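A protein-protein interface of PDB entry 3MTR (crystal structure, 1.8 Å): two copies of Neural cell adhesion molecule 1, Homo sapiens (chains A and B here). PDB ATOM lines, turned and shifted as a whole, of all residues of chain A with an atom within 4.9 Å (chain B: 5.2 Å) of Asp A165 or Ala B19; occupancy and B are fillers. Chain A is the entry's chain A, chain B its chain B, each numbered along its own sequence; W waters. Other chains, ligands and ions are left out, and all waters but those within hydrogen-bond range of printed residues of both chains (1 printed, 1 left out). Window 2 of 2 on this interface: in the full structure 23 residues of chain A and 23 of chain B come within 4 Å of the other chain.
The backbone NH (N) of Ala A166 sits at hydrogen-bond distance from the backbone carbonyl oxygen (O) of Leu A145 (3.1 Å).
The backbone NH of Lys A167 lies within hydrogen-bond range of the side-chain carboxylate of Asp A165 (2.6 Å).
The side-chain carboxylate (OD2) of Asp A165 is in hydrogen-bond range of the backbone NH (N) of Glu A168.
The backbone carbonyl oxygen (O) of Tyr B18 sits at hydrogen-bond distance from the side-chain amide nitrogen (ND2) of Asn B97 (2.9 Å).
NZ of Lys B21 is in hydrogen-bond range of O of Ala B19 (3.0 Å).
The backbone NH (N) of Lys B21 lies within hydrogen-bond range of the backbone carbonyl oxygen (O) of Phe B43 (2.9 Å).
Water W1 lies within hydrogen-bond range of the side-chain carboxylate (OD1) of Asp A165 (2.5 Å) and the backbone NH (N) of Ala B19 (2.8 Å).
Hydrophobic or aromatic side chains of chain A that line the printed part of chain B: Leu A145.
Of the 11 printed residues of chain B, 4 touch a printed residue of chain A.
Hydrophobic or aromatic side chains of chain B that line the printed part of chain A: Tyr B18 and Ala B19.
Among the printed residues, 5 pairs touch across the chains.
Among the printed residues, Asp or Glu carboxylates within 4 Å of a Lys or Arg side-chain nitrogen of the other chain: Asp A165 with Lys B21 (2.8 Å).
No position is printed for both chains.
Among the printed residues, merely in contact across the chains: Leu A145 with Tyr B18, Leu A145 with Lys B21 and Asp A165 with Ala B19.
Of the printed residues of chain B, Leu A145 touches Tyr B18 (3.5 Å) and Lys B21 (3.8 Å).
Of the printed residues of chain B, Lys A146 touches Met B17 (2.3 Å).
Tyr A164 touches none of the printed residues of chain B.
Asp A165 touches just these residues of chain B: Ala B19 (3.8 Å) and Lys B21 (2.8 Å).
Printed residues of chain A within 4 Å of Tyr B18: Leu A145.
Ala B19 touches just one residue of chain A: Asp A165.
Pro B20 touches none of the printed residues of chain A.
Of the printed residues of chain A, Lys B21 touches Leu A145 (3.8 Å) and Asp A165 (2.8 Å).
OD1 of Asp A165 lies within salt-bridge range of NZ of Lys B21, 2.8 Å away.
NZ of Lys A146 lies close to O of Met B17.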
ATOM      1  N   LEU A 145     -16.469  -0.079 -28.450  1.00  0.00           N
ATOM      2  CA  LEU A 145     -15.424  -1.050 -28.251  1.00  0.00           C
ATOM      3  C   LEU A 145     -15.727  -1.906 -27.039  1.00  0.00           C
ATOM      4  O   LEU A 145     -15.521  -3.143 -27.056  1.00  0.00           O
ATOM      5  CB  LEU A 145     -14.111  -0.328 -28.005  1.00  0.00           C
ATOM      6  CG  LEU A 145     -13.741   0.671 -29.094  1.00  0.00           C
ATOM      7  CD1 LEU A 145     -12.533   1.455 -28.664  1.00  0.00           C
ATOM      8  CD2 LEU A 145     -13.471  -0.094 -30.365  1.00  0.00           C
ATOM      9  N   LYS A 146     -16.212  -1.251 -25.988  1.00  0.00           N
ATOM     10  CA  LYS A 146     -16.566  -1.964 -24.759  1.00  0.00           C
ATOM     11  C   LYS A 146     -17.737  -1.355 -24.073  1.00  0.00           C
ATOM     12  O   LYS A 146     -18.098  -0.233 -24.384  1.00  0.00           O
ATOM     13  CB  LYS A 146     -15.429  -1.889 -23.750  1.00  0.00           C
ATOM     14  CG  LYS A 146     -14.187  -2.574 -24.144  1.00  0.00           C
ATOM     15  CD  LYS A 146     -13.398  -2.836 -22.859  1.00  0.00           C
ATOM     16  CE  LYS A 146     -11.998  -2.408 -23.015  1.00  0.00           C
ATOM     17  NZ  LYS A 146     -11.134  -3.163 -22.058  1.00  0.00           N
ATOM     18  N   TYR A 147     -18.267  -2.072 -23.068  1.00  0.00           N
ATOM     19  CA  TYR A 147     -19.243  -1.494 -22.150  1.00  0.00           C
ATOM     20  C   TYR A 147     -18.660  -1.581 -20.761  1.00  0.00           C
ATOM     21  O   TYR A 147     -17.923  -2.502 -20.483  1.00  0.00           O
ATOM     22  CB  TYR A 147     -20.557  -2.260 -22.212  1.00  0.00           C
ATOM     23  CG  TYR A 147     -21.338  -1.950 -23.478  1.00  0.00           C
ATOM     24  CD1 TYR A 147     -22.198  -0.872 -23.544  1.00  0.00           C
ATOM     25  CD2 TYR A 147     -21.181  -2.761 -24.610  1.00  0.00           C
ATOM     26  CE1 TYR A 147     -22.903  -0.570 -24.772  1.00  0.00           C
ATOM     27  CE2 TYR A 147     -21.863  -2.484 -25.807  1.00  0.00           C
ATOM     28  CZ  TYR A 147     -22.714  -1.392 -25.866  1.00  0.00           C
ATOM     29  OH  TYR A 147     -23.400  -1.117 -27.038  1.00  0.00           O
ATOM     30  N   TRP A 163     -15.888  -4.447 -16.986  1.00  0.00           N
ATOM     31  CA  TRP A 163     -15.888  -4.105 -18.419  1.00  0.00           C
ATOM     32  C   TRP A 163     -16.232  -5.325 -19.259  1.00  0.00           C
ATOM     33  O   TRP A 163     -15.892  -6.445 -18.883  1.00  0.00           O
ATOM     34  CB  TRP A 163     -14.498  -3.638 -18.818  1.00  0.00           C
ATOM     35  CG  TRP A 163     -14.156  -2.331 -18.222  1.00  0.00           C
ATOM     36  CD1 TRP A 163     -13.650  -2.093 -16.967  1.00  0.00           C
ATOM     37  CD2 TRP A 163     -14.309  -1.060 -18.845  1.00  0.00           C
ATOM     38  NE1 TRP A 163     -13.486  -0.733 -16.776  1.00  0.00           N
ATOM     39  CE2 TRP A 163     -13.886  -0.081 -17.916  1.00  0.00           C
ATOM     40  CE3 TRP A 163     -14.765  -0.642 -20.112  1.00  0.00           C
ATOM     41  CZ2 TRP A 163     -13.885   1.284 -18.219  1.00  0.00           C
ATOM     42  CZ3 TRP A 163     -14.770   0.707 -20.401  1.00  0.00           C
ATOM     43  CH2 TRP A 163     -14.324   1.656 -19.461  1.00  0.00           C
ATOM     44  N   TYR A 164     -16.899  -5.101 -20.383  1.00  0.00           N
ATOM     45  CA  TYR A 164     -17.334  -6.216 -21.258  1.00  0.00           C
ATOM     46  C   TYR A 164     -17.006  -5.891 -22.701  1.00  0.00           C
ATOM     47  O   TYR A 164     -17.188  -4.743 -23.111  1.00  0.00           O
ATOM     48  CB  TYR A 164     -18.843  -6.342 -21.163  1.00  0.00           C
ATOM     49  CG  TYR A 164     -19.340  -6.540 -19.755  1.00  0.00           C
ATOM     50  CD1 TYR A 164     -19.595  -7.816 -19.261  1.00  0.00           C
ATOM     51  CD2 TYR A 164     -19.563  -5.438 -18.926  1.00  0.00           C
ATOM     52  CE1 TYR A 164     -20.048  -7.991 -17.951  1.00  0.00           C
ATOM     53  CE2 TYR A 164     -20.022  -5.593 -17.629  1.00  0.00           C
ATOM     54  CZ  TYR A 164     -20.266  -6.859 -17.158  1.00  0.00           C
ATOM     55  OH  TYR A 164     -20.722  -6.979 -15.879  1.00  0.00           O
ATOM     56  N   ASP A 165     -16.603  -6.882 -23.494  1.00  0.00           N
ATOM     57  CA  ASP A 165     -16.376  -6.631 -24.924  1.00  0.00           C
ATOM     58  C   ASP A 165     -17.691  -6.269 -25.570  1.00  0.00           C
ATOM     59  O   ASP A 165     -18.720  -6.862 -25.256  1.00  0.00           O
ATOM     60  CB  ASP A 165     -15.794  -7.859 -25.622  1.00  0.00           C
ATOM     61  CG  ASP A 165     -15.608  -7.631 -27.117  1.00  0.00           C
ATOM     62  OD1 ASP A 165     -14.449  -7.479 -27.558  1.00  0.00           O
ATOM     63  OD2 ASP A 165     -16.628  -7.596 -27.854  1.00  0.00           O
ATOM     64  N   ALA A 166     -17.666  -5.323 -26.500  1.00  0.00           N
ATOM     65  CA  ALA A 166     -18.908  -4.754 -27.022  1.00  0.00           C
ATOM     66  C   ALA A 166     -19.616  -5.742 -27.931  1.00  0.00           C
ATOM     67  O   ALA A 166     -20.847  -5.736 -28.016  1.00  0.00           O
ATOM     68  CB  ALA A 166     -18.632  -3.492 -27.781  1.00  0.00           C
ATOM     69  N   LYS A 167     -18.836  -6.553 -28.631  1.00  0.00           N
ATOM     70  CA  LYS A 167     -19.420  -7.542 -29.537  1.00  0.00           C
ATOM     71  C   LYS A 167     -20.229  -8.609 -28.803  1.00  0.00           C
ATOM     72  O   LYS A 167     -21.401  -8.803 -29.126  1.00  0.00           O
ATOM     73  CB  LYS A 167     -18.381  -8.164 -30.476  1.00  0.00           C
ATOM     74  CG  LYS A 167     -18.939  -9.290 -31.345  1.00  0.00           C
ATOM     75  CD  LYS A 167     -17.838 -10.038 -32.100  1.00  0.00           C
ATOM     76  CE  LYS A 167     -18.083 -11.541 -32.059  1.00  0.00           C
ATOM     77  NZ  LYS A 167     -18.198 -12.009 -30.637  1.00  0.00           N
ATOM     78  N   GLU A 168     -19.634  -9.285 -27.821  1.00  0.00           N
ATOM     79  CA  GLU A 168     -20.381 -10.278 -27.041  1.00  0.00           C
ATOM     80  C   GLU A 168     -21.610  -9.662 -26.400  1.00  0.00           C
ATOM     81  O   GLU A 168     -22.678 -10.263 -26.386  1.00  0.00           O
ATOM     82  CB  GLU A 168     -19.546 -10.940 -25.932  1.00  0.00           C
ATOM     83  CG  GLU A 168     -20.344 -12.080 -25.264  1.00  0.00           C
ATOM     84  CD  GLU A 168     -19.536 -13.089 -24.410  1.00  0.00           C
ATOM     85  OE1 GLU A 168     -18.360 -13.401 -24.746  1.00  0.00           O
ATOM     86  OE2 GLU A 168     -20.130 -13.618 -23.428  1.00  0.00           O
ATOM     87  N   ALA A 169     -21.432  -8.466 -25.838  1.00  0.00           N
ATOM     88  CA  ALA A 169     -22.495  -7.788 -25.124  1.00  0.00           C
ATOM     89  C   ALA A 169     -23.646  -7.437 -26.081  1.00  0.00           C
ATOM     90  O   ALA A 169     -24.815  -7.775 -25.811  1.00  0.00           O
ATOM     91  CB  ALA A 169     -21.950  -6.529 -24.436  1.00  0.00           C
ATOM     92  N   MET B  17      -7.892  -2.010 -22.982  1.00  0.00           N
ATOM     93  CA  MET B  17      -7.585  -3.028 -24.040  1.00  0.00           C
ATOM     94  C   MET B  17      -8.839  -3.740 -24.528  1.00  0.00           C
ATOM     95  O   MET B  17      -9.755  -4.008 -23.760  1.00  0.00           O
ATOM     96  CB  MET B  17      -6.570  -4.049 -23.529  1.00  0.00           C
ATOM     97  CG  MET B  17      -5.235  -3.436 -23.184  1.00  0.00           C
ATOM     98  SD  MET B  17      -4.065  -4.674 -22.635  1.00  0.00           S
ATOM     99  CE  MET B  17      -3.912  -4.303 -20.882  1.00  0.00           C
ATOM    100  N   TYR B  18      -8.879  -4.059 -25.817  1.00  0.00           N
ATOM    101  CA  TYR B  18     -10.044  -4.713 -26.398  1.00  0.00           C
ATOM    102  C   TYR B  18      -9.615  -5.492 -27.624  1.00  0.00           C
ATOM    103  O   TYR B  18      -8.607  -5.165 -28.271  1.00  0.00           O
ATOM    104  CB  TYR B  18     -11.138  -3.684 -26.772  1.00  0.00           C
ATOM    105  CG  TYR B  18     -10.577  -2.452 -27.442  1.00  0.00           C
ATOM    106  CD1 TYR B  18     -10.511  -2.356 -28.829  1.00  0.00           C
ATOM    107  CD2 TYR B  18     -10.050  -1.400 -26.679  1.00  0.00           C
ATOM    108  CE1 TYR B  18      -9.971  -1.229 -29.450  1.00  0.00           C
ATOM    109  CE2 TYR B  18      -9.502  -0.274 -27.296  1.00  0.00           C
ATOM    110  CZ  TYR B  18      -9.468  -0.204 -28.672  1.00  0.00           C
ATOM    111  OH  TYR B  18      -8.933   0.896 -29.289  1.00  0.00           O
ATOM    112  N   ALA B  19     -10.399  -6.514 -27.943  1.00  0.00           N
ATOM    113  CA  ALA B  19     -10.235  -7.249 -29.183  1.00  0.00           C
ATOM    114  C   ALA B  19     -10.520  -6.309 -30.358  1.00  0.00           C
ATOM    115  O   ALA B  19     -11.212  -5.303 -30.198  1.00  0.00           O
ATOM    116  CB  ALA B  19     -11.155  -8.461 -29.212  1.00  0.00           C
ATOM    117  N   PRO B  20      -9.936  -6.608 -31.524  1.00  0.00           N
ATOM    118  CA  PRO B  20     -10.073  -5.731 -32.686  1.00  0.00           C
ATOM    119  C   PRO B  20     -11.506  -5.622 -33.144  1.00  0.00           C
ATOM    120  O   PRO B  20     -12.255  -6.609 -33.086  1.00  0.00           O
ATOM    121  CB  PRO B  20      -9.188  -6.416 -33.743  1.00  0.00           C
ATOM    122  CG  PRO B  20      -8.270  -7.252 -32.972  1.00  0.00           C
ATOM    123  CD  PRO B  20      -9.107  -7.773 -31.837  1.00  0.00           C
ATOM    124  N   LYS B  21     -11.889  -4.415 -33.578  1.00  0.00           N
ATOM    125  CA  LYS B  21     -13.154  -4.178 -34.250  1.00  0.00           C
ATOM    126  C   LYS B  21     -12.821  -3.764 -35.676  1.00  0.00           C
ATOM    127  O   LYS B  21     -11.853  -3.042 -35.885  1.00  0.00           O
ATOM    128  CB  LYS B  21     -13.939  -3.067 -33.532  1.00  0.00           C
ATOM    129  CG  LYS B  21     -14.246  -3.382 -32.057  1.00  0.00           C
ATOM    130  CD  LYS B  21     -15.133  -4.614 -31.865  1.00  0.00           C
ATOM    131  CE  LYS B  21     -15.211  -5.043 -30.384  1.00  0.00           C
ATOM    132  NZ  LYS B  21     -14.096  -5.929 -29.903  1.00  0.00           N
ATOM    133  N   PHE B  43      -9.696  -1.117 -35.423  1.00  0.00           N
ATOM    134  CA  PHE B  43      -9.599  -0.387 -34.162  1.00  0.00           C
ATOM    135  C   PHE B  43      -9.208  -1.437 -33.179  1.00  0.00           C
ATOM    136  O   PHE B  43      -9.954  -2.380 -32.987  1.00  0.00           O
ATOM    137  CB  PHE B  43     -10.973   0.141 -33.791  1.00  0.00           C
ATOM    138  CG  PHE B  43     -11.465   1.229 -34.733  1.00  0.00           C
ATOM    139  CD1 PHE B  43     -11.181   2.559 -34.456  1.00  0.00           C
ATOM    140  CD2 PHE B  43     -12.175   0.916 -35.869  1.00  0.00           C
ATOM    141  CE1 PHE B  43     -11.605   3.574 -35.300  1.00  0.00           C
ATOM    142  CE2 PHE B  43     -12.584   1.927 -36.741  1.00  0.00           C
ATOM    143  CZ  PHE B  43     -12.308   3.264 -36.425  1.00  0.00           C
ATOM    144  N   ALA B  44      -8.037  -1.306 -32.574  1.00  0.00           N
ATOM    145  CA  ALA B  44      -7.594  -2.291 -31.627  1.00  0.00           C
ATOM    146  C   ALA B  44      -6.518  -1.672 -30.759  1.00  0.00           C
ATOM    147  O   ALA B  44      -5.698  -0.890 -31.253  1.00  0.00           O
ATOM    148  CB  ALA B  44      -7.028  -3.493 -32.355  1.00  0.00           C
ATOM    149  N   ASN B  97      -5.115  -9.413 -31.952  1.00  0.00           N
ATOM    150  CA  ASN B  97      -4.176  -8.829 -31.033  1.00  0.00           C
ATOM    151  C   ASN B  97      -4.139  -9.709 -29.785  1.00  0.00           C
ATOM    152  O   ASN B  97      -4.694 -10.820 -29.771  1.00  0.00           O
ATOM    153  CB  ASN B  97      -4.529  -7.357 -30.730  1.00  0.00           C
ATOM    154  CG  ASN B  97      -5.779  -7.221 -29.860  1.00  0.00           C
ATOM    155  OD1 ASN B  97      -6.413  -8.224 -29.540  1.00  0.00           O
ATOM    156  ND2 ASN B  97      -6.151  -5.970 -29.485  1.00  0.00           N
ATOM    157  N   ILE B  99      -5.740  -9.685 -27.220  1.00  0.00           N
ATOM    158  CA  ILE B  99      -7.003  -9.897 -26.494  1.00  0.00           C
ATOM    159  C   ILE B  99      -7.931 -10.832 -27.261  1.00  0.00           C
ATOM    160  O   ILE B  99      -8.652 -11.625 -26.673  1.00  0.00           O
ATOM    161  CB  ILE B  99      -7.740  -8.574 -26.155  1.00  0.00           C
ATOM    162  CG1 ILE B  99      -6.799  -7.557 -25.497  1.00  0.00           C
ATOM    163  CG2 ILE B  99      -8.974  -8.828 -25.258  1.00  0.00           C
ATOM    164  CD1 ILE B  99      -6.110  -8.009 -24.165  1.00  0.00           C
ATOM    165  N   GLY B 100      -7.887 -10.771 -28.580  1.00  0.00           N
ATOM    166  CA  GLY B 100      -8.768 -11.633 -29.341  1.00  0.00           C
ATOM    167  C   GLY B 100      -8.623 -11.443 -30.829  1.00  0.00           C
ATOM    168  O   GLY B 100      -7.630 -10.893 -31.287  1.00  0.00           O
ATOM    169  N   GLN B 101      -9.652 -11.863 -31.571  1.00  0.00           N
ATOM    170  CA  GLN B 101      -9.574 -11.955 -33.030  1.00  0.00           C
ATOM    171  C   GLN B 101     -10.936 -11.586 -33.593  1.00  0.00           C
ATOM    172  O   GLN B 101     -11.959 -11.834 -32.947  1.00  0.00           O
ATOM    173  CB  GLN B 101      -9.212 -13.389 -33.449  1.00  0.00           C
ATOM    174  CG  GLN B 101      -7.943 -14.010 -32.793  1.00  0.00           C
ATOM    175  CD  GLN B 101      -7.673 -15.458 -33.236  1.00  0.00           C
ATOM    176  OE1 GLN B 101      -7.929 -15.827 -34.385  1.00  0.00           O
ATOM    177  NE2 GLN B 101      -7.146 -16.267 -32.340  1.00  0.00           N
HETATM  178  O   HOH W   1     -12.462  -7.119 -26.157  1.00  0.00           O
